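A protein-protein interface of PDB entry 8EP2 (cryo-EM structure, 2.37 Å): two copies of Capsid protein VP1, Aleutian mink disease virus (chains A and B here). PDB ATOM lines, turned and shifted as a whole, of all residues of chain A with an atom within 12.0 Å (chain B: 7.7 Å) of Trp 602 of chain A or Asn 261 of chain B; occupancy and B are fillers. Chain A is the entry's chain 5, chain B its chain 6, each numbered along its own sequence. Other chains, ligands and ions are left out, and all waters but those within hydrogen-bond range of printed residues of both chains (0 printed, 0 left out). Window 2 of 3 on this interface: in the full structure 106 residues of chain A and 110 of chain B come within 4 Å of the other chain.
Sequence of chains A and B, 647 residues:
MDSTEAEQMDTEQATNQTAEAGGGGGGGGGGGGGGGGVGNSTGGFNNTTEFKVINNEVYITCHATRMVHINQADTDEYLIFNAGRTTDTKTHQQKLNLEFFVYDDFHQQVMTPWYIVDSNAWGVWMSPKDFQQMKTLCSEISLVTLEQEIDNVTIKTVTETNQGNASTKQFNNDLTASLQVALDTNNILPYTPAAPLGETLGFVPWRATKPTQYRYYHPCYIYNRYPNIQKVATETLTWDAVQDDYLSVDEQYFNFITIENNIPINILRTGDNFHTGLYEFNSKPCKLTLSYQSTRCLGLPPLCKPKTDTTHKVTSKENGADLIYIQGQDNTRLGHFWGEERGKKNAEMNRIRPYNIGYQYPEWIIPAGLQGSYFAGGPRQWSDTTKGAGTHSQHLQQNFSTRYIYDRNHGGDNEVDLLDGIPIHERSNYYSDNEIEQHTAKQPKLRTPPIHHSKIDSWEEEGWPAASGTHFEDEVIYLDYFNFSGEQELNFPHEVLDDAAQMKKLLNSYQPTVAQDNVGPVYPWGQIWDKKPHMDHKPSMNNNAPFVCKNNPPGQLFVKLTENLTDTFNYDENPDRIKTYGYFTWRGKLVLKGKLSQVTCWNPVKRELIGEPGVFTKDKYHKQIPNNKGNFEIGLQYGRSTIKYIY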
ATOM      1  N   GLN A 598       2.445  16.069   9.476  1.00  0.00           N
ATOM      2  CA  GLN A 598       1.954  14.769   9.056  1.00  0.00           C
ATOM      3  C   GLN A 598       2.551  14.489   7.689  1.00  0.00           C
ATOM      4  O   GLN A 598       2.165  15.115   6.699  1.00  0.00           O
ATOM      5  CB  GLN A 598       0.433  14.751   9.011  1.00  0.00           C
ATOM      6  CG  GLN A 598      -0.125  13.389   8.750  1.00  0.00           C
ATOM      7  CD  GLN A 598       0.241  12.433   9.850  1.00  0.00           C
ATOM      8  OE1 GLN A 598      -0.074  12.670  11.012  1.00  0.00           O
ATOM      9  NE2 GLN A 598       0.912  11.345   9.495  1.00  0.00           N
ATOM     10  N   VAL A 599       3.483  13.557   7.637  1.00  0.00           N
ATOM     11  CA  VAL A 599       4.110  13.147   6.394  1.00  0.00           C
ATOM     12  C   VAL A 599       3.508  11.812   6.007  1.00  0.00           C
ATOM     13  O   VAL A 599       3.347  10.932   6.855  1.00  0.00           O
ATOM     14  CB  VAL A 599       5.634  13.057   6.541  1.00  0.00           C
ATOM     15  CG1 VAL A 599       6.239  12.516   5.287  1.00  0.00           C
ATOM     16  CG2 VAL A 599       6.193  14.419   6.837  1.00  0.00           C
ATOM     17  N   THR A 600       3.077  11.701   4.764  1.00  0.00           N
ATOM     18  CA  THR A 600       2.348  10.533   4.309  1.00  0.00           C
ATOM     19  C   THR A 600       3.164   9.554   3.475  1.00  0.00           C
ATOM     20  O   THR A 600       2.623   8.530   3.063  1.00  0.00           O
ATOM     21  CB  THR A 600       1.121  10.993   3.543  1.00  0.00           C
ATOM     22  OG1 THR A 600       1.531  11.810   2.447  1.00  0.00           O
ATOM     23  CG2 THR A 600       0.266  11.821   4.462  1.00  0.00           C
ATOM     24  N   CYS A 601       4.432   9.828   3.204  1.00  0.00           N
ATOM     25  CA  CYS A 601       5.166   8.979   2.281  1.00  0.00           C
ATOM     26  C   CYS A 601       5.613   7.682   2.948  1.00  0.00           C
ATOM     27  O   CYS A 601       5.683   7.568   4.169  1.00  0.00           O
ATOM     28  CB  CYS A 601       6.379   9.704   1.709  1.00  0.00           C
ATOM     29  SG  CYS A 601       7.559  10.277   2.911  1.00  0.00           S
ATOM     30  N   TRP A 602       5.885   6.682   2.112  1.00  0.00           N
ATOM     31  CA  TRP A 602       6.438   5.421   2.591  1.00  0.00           C
ATOM     32  C   TRP A 602       7.898   5.568   2.984  1.00  0.00           C
ATOM     33  O   TRP A 602       8.299   5.184   4.085  1.00  0.00           O
ATOM     34  CB  TRP A 602       6.294   4.361   1.508  1.00  0.00           C
ATOM     35  CG  TRP A 602       7.051   3.110   1.763  1.00  0.00           C
ATOM     36  CD1 TRP A 602       8.268   2.792   1.270  1.00  0.00           C
ATOM     37  CD2 TRP A 602       6.621   1.985   2.518  1.00  0.00           C
ATOM     38  NE1 TRP A 602       8.644   1.557   1.695  1.00  0.00           N
ATOM     39  CE2 TRP A 602       7.644   1.034   2.463  1.00  0.00           C
ATOM     40  CE3 TRP A 602       5.475   1.694   3.252  1.00  0.00           C
ATOM     41  CZ2 TRP A 602       7.561  -0.182   3.105  1.00  0.00           C
ATOM     42  CZ3 TRP A 602       5.395   0.491   3.887  1.00  0.00           C
ATOM     43  CH2 TRP A 602       6.427  -0.435   3.812  1.00  0.00           C
ATOM     44  N   ASN A 603       8.708   6.105   2.084  1.00  0.00           N
ATOM     45  CA  ASN A 603      10.131   6.234   2.302  1.00  0.00           C
ATOM     46  C   ASN A 603      10.432   7.214   3.424  1.00  0.00           C
ATOM     47  O   ASN A 603       9.625   8.086   3.736  1.00  0.00           O
ATOM     48  CB  ASN A 603      10.800   6.697   1.021  1.00  0.00           C
ATOM     49  CG  ASN A 603      10.107   7.894   0.421  1.00  0.00           C
ATOM     50  OD1 ASN A 603       8.921   8.101   0.641  1.00  0.00           O
ATOM     51  ND2 ASN A 603      10.846   8.715  -0.290  1.00  0.00           N
ATOM     52  N   PRO A 604      11.596   7.089   4.049  1.00  0.00           N
ATOM     53  CA  PRO A 604      12.014   8.088   5.030  1.00  0.00           C
ATOM     54  C   PRO A 604      12.371   9.408   4.368  1.00  0.00           C
ATOM     55  O   PRO A 604      12.818   9.454   3.222  1.00  0.00           O
ATOM     56  CB  PRO A 604      13.231   7.439   5.692  1.00  0.00           C
ATOM     57  CG  PRO A 604      13.722   6.482   4.702  1.00  0.00           C
ATOM     58  CD  PRO A 604      12.525   5.955   4.002  1.00  0.00           C
ATOM     59  N   VAL A 605      12.173  10.488   5.107  1.00  0.00           N
ATOM     60  CA  VAL A 605      12.278  11.836   4.566  1.00  0.00           C
ATOM     61  C   VAL A 605      13.653  12.404   4.856  1.00  0.00           C
ATOM     62  O   VAL A 605      14.266  12.133   5.890  1.00  0.00           O
ATOM     63  CB  VAL A 605      11.183  12.764   5.128  1.00  0.00           C
ATOM     64  CG1 VAL A 605       9.836  12.241   4.765  1.00  0.00           C
ATOM     65  CG2 VAL A 605      11.310  12.893   6.620  1.00  0.00           C
ATOM     66  N   LYS A 606      14.145  13.201   3.923  1.00  0.00           N
ATOM     67  CA  LYS A 606      15.414  13.901   4.060  1.00  0.00           C
ATOM     68  C   LYS A 606      15.119  15.385   4.197  1.00  0.00           C
ATOM     69  O   LYS A 606      14.687  16.024   3.239  1.00  0.00           O
ATOM     70  CB  LYS A 606      16.308  13.625   2.858  1.00  0.00           C
ATOM     71  CG  LYS A 606      17.632  14.319   2.932  1.00  0.00           C
ATOM     72  CD  LYS A 606      18.441  13.805   4.095  1.00  0.00           C
ATOM     73  CE  LYS A 606      19.783  14.500   4.155  1.00  0.00           C
ATOM     74  NZ  LYS A 606      20.606  14.176   2.959  1.00  0.00           N
ATOM     75  N   ARG A 607      15.345  15.932   5.387  1.00  0.00           N
ATOM     76  CA  ARG A 607      14.953  17.300   5.694  1.00  0.00           C
ATOM     77  C   ARG A 607      16.083  18.306   5.542  1.00  0.00           C
ATOM     78  O   ARG A 607      15.895  19.475   5.871  1.00  0.00           O
ATOM     79  CB  ARG A 607      14.390  17.384   7.107  1.00  0.00           C
ATOM     80  CG  ARG A 607      13.137  16.585   7.308  1.00  0.00           C
ATOM     81  CD  ARG A 607      12.645  16.718   8.724  1.00  0.00           C
ATOM     82  NE  ARG A 607      11.554  15.798   9.004  1.00  0.00           N
ATOM     83  CZ  ARG A 607      10.285  16.059   8.751  1.00  0.00           C
ATOM     84  NH1 ARG A 607       9.945  17.218   8.220  1.00  0.00           N
ATOM     85  NH2 ARG A 607       9.357  15.164   9.035  1.00  0.00           N
ATOM     86  N   THR A 642      10.529  20.257   4.053  1.00  0.00           N
ATOM     87  CA  THR A 642       9.845  18.986   3.872  1.00  0.00           C
ATOM     88  C   THR A 642       9.052  19.013   2.578  1.00  0.00           C
ATOM     89  O   THR A 642       8.361  19.991   2.291  1.00  0.00           O
ATOM     90  CB  THR A 642       8.930  18.687   5.056  1.00  0.00           C
ATOM     91  OG1 THR A 642       9.714  18.630   6.248  1.00  0.00           O
ATOM     92  CG2 THR A 642       8.249  17.359   4.875  1.00  0.00           C
ATOM     93  N   ILE A 643       9.155  17.948   1.809  1.00  0.00           N
ATOM     94  CA  ILE A 643       8.489  17.879   0.518  1.00  0.00           C
ATOM     95  C   ILE A 643       7.016  17.567   0.722  1.00  0.00           C
ATOM     96  O   ILE A 643       6.642  16.773   1.589  1.00  0.00           O
ATOM     97  CB  ILE A 643       9.173  16.841  -0.384  1.00  0.00           C
ATOM     98  CG1 ILE A 643       8.610  16.920  -1.792  1.00  0.00           C
ATOM     99  CG2 ILE A 643       9.012  15.448   0.165  1.00  0.00           C
ATOM    100  CD1 ILE A 643       8.915  18.208  -2.469  1.00  0.00           C
ATOM    101  N   LYS A 644       6.166  18.223  -0.059  1.00  0.00           N
ATOM    102  CA  LYS A 644       4.735  17.993   0.011  1.00  0.00           C
ATOM    103  C   LYS A 644       4.129  18.332  -1.339  1.00  0.00           C
ATOM    104  O   LYS A 644       4.633  19.194  -2.056  1.00  0.00           O
ATOM    105  CB  LYS A 644       4.102  18.827   1.122  1.00  0.00           C
ATOM    106  CG  LYS A 644       2.639  18.577   1.359  1.00  0.00           C
ATOM    107  CD  LYS A 644       2.206  19.235   2.641  1.00  0.00           C
ATOM    108  CE  LYS A 644       0.738  19.026   2.921  1.00  0.00           C
ATOM    109  NZ  LYS A 644      -0.122  19.841   2.031  1.00  0.00           N
ATOM    110  N   TYR A 645       3.056  17.640  -1.689  1.00  0.00           N
ATOM    111  CA  TYR A 645       2.312  17.977  -2.892  1.00  0.00           C
ATOM    112  C   TYR A 645       1.475  19.218  -2.661  1.00  0.00           C
ATOM    113  O   TYR A 645       0.664  19.263  -1.737  1.00  0.00           O
ATOM    114  CB  TYR A 645       1.405  16.831  -3.321  1.00  0.00           C
ATOM    115  CG  TYR A 645       2.103  15.716  -4.018  1.00  0.00           C
ATOM    116  CD1 TYR A 645       2.275  15.753  -5.382  1.00  0.00           C
ATOM    117  CD2 TYR A 645       2.582  14.627  -3.326  1.00  0.00           C
ATOM    118  CE1 TYR A 645       2.903  14.747  -6.035  1.00  0.00           C
ATOM    119  CE2 TYR A 645       3.215  13.613  -3.974  1.00  0.00           C
ATOM    120  CZ  TYR A 645       3.376  13.681  -5.327  1.00  0.00           C
ATOM    121  OH  TYR A 645       4.012  12.671  -5.991  1.00  0.00           O
ATOM    122  N   TYR B  78       2.452  -1.428  -6.318  1.00  0.00           N
ATOM    123  CA  TYR B  78       2.655  -0.057  -6.748  1.00  0.00           C
ATOM    124  C   TYR B  78       3.830   0.001  -7.707  1.00  0.00           C
ATOM    125  O   TYR B  78       4.853  -0.647  -7.493  1.00  0.00           O
ATOM    126  CB  TYR B  78       2.908   0.848  -5.549  1.00  0.00           C
ATOM    127  CG  TYR B  78       1.687   1.137  -4.724  1.00  0.00           C
ATOM    128  CD1 TYR B  78       0.921   2.255  -4.972  1.00  0.00           C
ATOM    129  CD2 TYR B  78       1.291   0.290  -3.712  1.00  0.00           C
ATOM    130  CE1 TYR B  78      -0.187   2.535  -4.226  1.00  0.00           C
ATOM    131  CE2 TYR B  78       0.177   0.558  -2.967  1.00  0.00           C
ATOM    132  CZ  TYR B  78      -0.560   1.682  -3.228  1.00  0.00           C
ATOM    133  OH  TYR B  78      -1.675   1.954  -2.479  1.00  0.00           O
ATOM    134  N   ILE B 188      -5.288  13.361   1.470  1.00  0.00           N
ATOM    135  CA  ILE B 188      -3.882  13.033   1.645  1.00  0.00           C
ATOM    136  C   ILE B 188      -3.226  12.754   0.305  1.00  0.00           C
ATOM    137  O   ILE B 188      -2.090  13.164   0.058  1.00  0.00           O
ATOM    138  CB  ILE B 188      -3.756  11.840   2.601  1.00  0.00           C
ATOM    139  CG1 ILE B 188      -4.028  12.283   4.032  1.00  0.00           C
ATOM    140  CG2 ILE B 188      -2.433  11.149   2.437  1.00  0.00           C
ATOM    141  CD1 ILE B 188      -4.147  11.139   4.992  1.00  0.00           C
ATOM    142  N   PHE B 254      11.904  12.246  -3.490  1.00  0.00           N
ATOM    143  CA  PHE B 254      10.986  11.116  -3.541  1.00  0.00           C
ATOM    144  C   PHE B 254       9.870  11.290  -2.534  1.00  0.00           C
ATOM    145  O   PHE B 254      10.117  11.430  -1.337  1.00  0.00           O
ATOM    146  CB  PHE B 254      11.714   9.806  -3.272  1.00  0.00           C
ATOM    147  CG  PHE B 254      12.585   9.365  -4.384  1.00  0.00           C
ATOM    148  CD1 PHE B 254      12.431   9.892  -5.639  1.00  0.00           C
ATOM    149  CD2 PHE B 254      13.537   8.394  -4.183  1.00  0.00           C
ATOM    150  CE1 PHE B 254      13.223   9.481  -6.664  1.00  0.00           C
ATOM    151  CE2 PHE B 254      14.330   7.979  -5.209  1.00  0.00           C
ATOM    152  CZ  PHE B 254      14.173   8.523  -6.450  1.00  0.00           C
ATOM    153  N   ASN B 255       8.642  11.291  -3.022  1.00  0.00           N
ATOM    154  CA  ASN B 255       7.466  11.307  -2.168  1.00  0.00           C
ATOM    155  C   ASN B 255       6.545  10.229  -2.715  1.00  0.00           C
ATOM    156  O   ASN B 255       5.915  10.417  -3.757  1.00  0.00           O
ATOM    157  CB  ASN B 255       6.839  12.694  -2.185  1.00  0.00           C
ATOM    158  CG  ASN B 255       5.827  12.892  -1.103  1.00  0.00           C
ATOM    159  OD1 ASN B 255       5.817  12.176  -0.115  1.00  0.00           O
ATOM    160  ND2 ASN B 255       5.013  13.919  -1.247  1.00  0.00           N
ATOM    161  N   PHE B 256       6.425   9.124  -1.999  1.00  0.00           N
ATOM    162  CA  PHE B 256       5.720   7.948  -2.492  1.00  0.00           C
ATOM    163  C   PHE B 256       4.666   7.547  -1.479  1.00  0.00           C
ATOM    164  O   PHE B 256       4.989   7.089  -0.380  1.00  0.00           O
ATOM    165  CB  PHE B 256       6.699   6.818  -2.783  1.00  0.00           C
ATOM    166  CG  PHE B 256       6.066   5.475  -2.830  1.00  0.00           C
ATOM    167  CD1 PHE B 256       5.130   5.164  -3.783  1.00  0.00           C
ATOM    168  CD2 PHE B 256       6.462   4.495  -1.954  1.00  0.00           C
ATOM    169  CE1 PHE B 256       4.558   3.927  -3.816  1.00  0.00           C
ATOM    170  CE2 PHE B 256       5.902   3.255  -1.995  1.00  0.00           C
ATOM    171  CZ  PHE B 256       4.951   2.970  -2.926  1.00  0.00           C
ATOM    172  N   ILE B 257       3.409   7.697  -1.864  1.00  0.00           N
ATOM    173  CA  ILE B 257       2.285   7.645  -0.948  1.00  0.00           C
ATOM    174  C   ILE B 257       1.386   6.506  -1.379  1.00  0.00           C
ATOM    175  O   ILE B 257       1.079   6.371  -2.564  1.00  0.00           O
ATOM    176  CB  ILE B 257       1.521   8.975  -0.943  1.00  0.00           C
ATOM    177  CG1 ILE B 257       2.459  10.097  -0.529  1.00  0.00           C
ATOM    178  CG2 ILE B 257       0.359   8.914   0.005  1.00  0.00           C
ATOM    179  CD1 ILE B 257       1.899  11.455  -0.751  1.00  0.00           C
ATOM    180  N   THR B 258       0.968   5.690  -0.426  1.00  0.00           N
ATOM    181  CA  THR B 258       0.082   4.577  -0.701  1.00  0.00           C
ATOM    182  C   THR B 258      -1.241   4.795  -0.002  1.00  0.00           C
ATOM    183  O   THR B 258      -1.338   5.524   0.984  1.00  0.00           O
ATOM    184  CB  THR B 258       0.674   3.251  -0.234  1.00  0.00           C
ATOM    185  OG1 THR B 258       0.826   3.274   1.186  1.00  0.00           O
ATOM    186  CG2 THR B 258       2.013   3.025  -0.868  1.00  0.00           C
ATOM    187  N   ILE B 259      -2.267   4.145  -0.530  1.00  0.00           N
ATOM    188  CA  ILE B 259      -3.565   4.182   0.120  1.00  0.00           C
ATOM    189  C   ILE B 259      -3.539   3.372   1.404  1.00  0.00           C
ATOM    190  O   ILE B 259      -4.079   3.794   2.429  1.00  0.00           O
ATOM    191  CB  ILE B 259      -4.642   3.693  -0.862  1.00  0.00           C
ATOM    192  CG1 ILE B 259      -4.809   4.725  -1.966  1.00  0.00           C
ATOM    193  CG2 ILE B 259      -5.939   3.446  -0.158  1.00  0.00           C
ATOM    194  CD1 ILE B 259      -5.662   4.292  -3.085  1.00  0.00           C
ATOM    195  N   GLU B 260      -2.868   2.223   1.383  1.00  0.00           N
ATOM    196  CA  GLU B 260      -2.914   1.300   2.509  1.00  0.00           C
ATOM    197  C   GLU B 260      -2.326   1.885   3.780  1.00  0.00           C
ATOM    198  O   GLU B 260      -2.767   1.526   4.872  1.00  0.00           O
ATOM    199  CB  GLU B 260      -2.199   0.009   2.146  1.00  0.00           C
ATOM    200  CG  GLU B 260      -2.992  -0.861   1.215  1.00  0.00           C
ATOM    201  CD  GLU B 260      -2.965  -0.391  -0.217  1.00  0.00           C
ATOM    202  OE1 GLU B 260      -2.374   0.670  -0.502  1.00  0.00           O
ATOM    203  OE2 GLU B 260      -3.550  -1.089  -1.067  1.00  0.00           O
ATOM    204  N   ASN B 261      -1.337   2.760   3.682  1.00  0.00           N
ATOM    205  CA  ASN B 261      -0.799   3.341   4.901  1.00  0.00           C
ATOM    206  C   ASN B 261      -1.665   4.457   5.451  1.00  0.00           C
ATOM    207  O   ASN B 261      -1.730   4.638   6.666  1.00  0.00           O
ATOM    208  CB  ASN B 261       0.610   3.867   4.669  1.00  0.00           C
ATOM    209  CG  ASN B 261       1.617   2.768   4.505  1.00  0.00           C
ATOM    210  OD1 ASN B 261       2.371   2.745   3.543  1.00  0.00           O
ATOM    211  ND2 ASN B 261       1.659   1.859   5.460  1.00  0.00           N
ATOM    212  N   ASN B 262      -2.253   5.268   4.587  1.00  0.00           N
ATOM    213  CA  ASN B 262      -2.929   6.480   5.014  1.00  0.00           C
ATOM    214  C   ASN B 262      -4.413   6.338   5.316  1.00  0.00           C
ATOM    215  O   ASN B 262      -4.916   7.039   6.195  1.00  0.00           O
ATOM    216  CB  ASN B 262      -2.681   7.552   3.973  1.00  0.00           C
ATOM    217  CG  ASN B 262      -1.234   7.914   3.913  1.00  0.00           C
ATOM    218  OD1 ASN B 262      -0.734   8.631   4.765  1.00  0.00           O
ATOM    219  ND2 ASN B 262      -0.530   7.365   2.943  1.00  0.00           N
ATOM    220  N   ILE B 263      -5.149   5.483   4.617  1.00  0.00           N
ATOM    221  CA  ILE B 263      -6.604   5.511   4.754  1.00  0.00           C
ATOM    222  C   ILE B 263      -7.124   4.177   5.268  1.00  0.00           C
ATOM    223  O   ILE B 263      -6.635   3.123   4.856  1.00  0.00           O
ATOM    224  CB  ILE B 263      -7.272   5.857   3.416  1.00  0.00           C
ATOM    225  CG1 ILE B 263      -6.875   7.252   2.960  1.00  0.00           C
ATOM    226  CG2 ILE B 263      -8.768   5.792   3.522  1.00  0.00           C
ATOM    227  CD1 ILE B 263      -5.835   7.241   1.914  1.00  0.00           C
ATOM    228  N   PRO B 264      -8.119   4.174   6.150  1.00  0.00           N
ATOM    229  CA  PRO B 264      -8.777   2.917   6.509  1.00  0.00           C
ATOM    230  C   PRO B 264      -9.633   2.416   5.358  1.00  0.00           C
ATOM    231  O   PRO B 264     -10.278   3.197   4.659  1.00  0.00           O
ATOM    232  CB  PRO B 264      -9.638   3.305   7.712  1.00  0.00           C
ATOM    233  CG  PRO B 264      -8.994   4.518   8.246  1.00  0.00           C
ATOM    234  CD  PRO B 264      -8.497   5.259   7.060  1.00  0.00           C
ATOM    235  N   ILE B 265      -9.651   1.106   5.170  1.00  0.00           N
ATOM    236  CA  ILE B 265     -10.259   0.494   3.999  1.00  0.00           C
ATOM    237  C   ILE B 265     -11.460  -0.333   4.422  1.00  0.00           C
ATOM    238  O   ILE B 265     -11.420  -1.032   5.437  1.00  0.00           O
ATOM    239  CB  ILE B 265      -9.228  -0.362   3.246  1.00  0.00           C
ATOM    240  CG1 ILE B 265      -8.124   0.535   2.702  1.00  0.00           C
ATOM    241  CG2 ILE B 265      -9.877  -1.111   2.120  1.00  0.00           C
ATOM    242  CD1 ILE B 265      -6.938  -0.209   2.191  1.00  0.00           C
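No position is printed for both chains.
O of Thr 600 of chain A is in hydrogen-bond range of ND2 of Asn 262 of chain B (3.4 Å). The backbone NH (N) of Trp 602 of chain A is in hydrogen-bond range of the backbone carbonyl oxygen (O) of Phe 256 of chain B (2.7 Å). The backbone carbonyl oxygen of Phe 254 of chain B sits at hydrogen-bond distance from the side-chain amide nitrogen of Asn 603 of chain A (3.0 Å).
Of the printed residues of chain B, Cys 601 of chain A touches Asn 255 and Phe 256. Trp 602 of chain A touches just these residues of chain B: Phe 256 and Asn 261. Printed residues of chain B within 4 Å of Asn 603 of chain A: Phe 254 (3.0 Å) and Phe 256 (3.8 Å). Pro 604 of chain A touches none of the printed residues of chain B. Thr 642 of chain A touches none of the printed residues of chain B. Of the printed residues of chain A, Asn 255 of chain B touches Cys 601 (3.1 Å) and Tyr 645 (3.3 Å). Of chain A, only Cys 601, Trp 602 and Asn 603 come within 4 Å of Phe 256 of chain B. Of chain A, only Thr 600 (3.2 Å) comes within 4 Å of Ile 257 of chain B. No residue of chain A comes within 4 Å of Thr 258 of chain B. Glu 260 of chain B touches none of the printed residues of chain A. Of chain A, only Thr 600 (3.2 Å) comes within 4 Å of Asn 262 of chain B. Ile 263 of chain B touches none of the printed residues of chain A. The nearest residue of chain B that does not touch Trp 602 of chain A is Ile 257 of chain B (4.8 Å).
Printed residues of chain A that touch a printed residue of chain B: Thr 600, Cys 601, Trp 602, Asn 603 and Tyr 645. Hydrophobic or aromatic side chains of chain A that line the printed part of chain B: Trp 602 and Tyr 645. Of the 14 printed residues of chain B, 7 touch a printed residue of chain A.
The backbone carbonyl oxygen of Asn 603 of chain A lies within hydrogen-bond range of the side-chain sulfur of Cys 601 of chain A (3.1 Å). OG1 of Thr 258 of chain B lies within hydrogen-bond range of OD1 of Asn 261 of chain B (2.9 Å). O of Thr 258 of chain B is in hydrogen-bond range of ND2 of Asn 262 of chain B.
Among the printed residues, pairs that only touch across the chains: Thr 600 of chain A with Ile 188 of chain B (3.4 Å), Thr 600 of chain A with Ile 257 of chain B (3.2 Å), Cys 601 of chain A with Asn 255 of chain B (3.1 Å), Cys 601 of chain A with Phe 256 of chain B (3.3 Å), Trp 602 of chain A with Asn 261 of chain B (3.3 Å), Asn 603 of chain A with Phe 256 of chain B (3.8 Å) and Tyr 645 of chain A with Asn 255 of chain B (3.3 Å).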
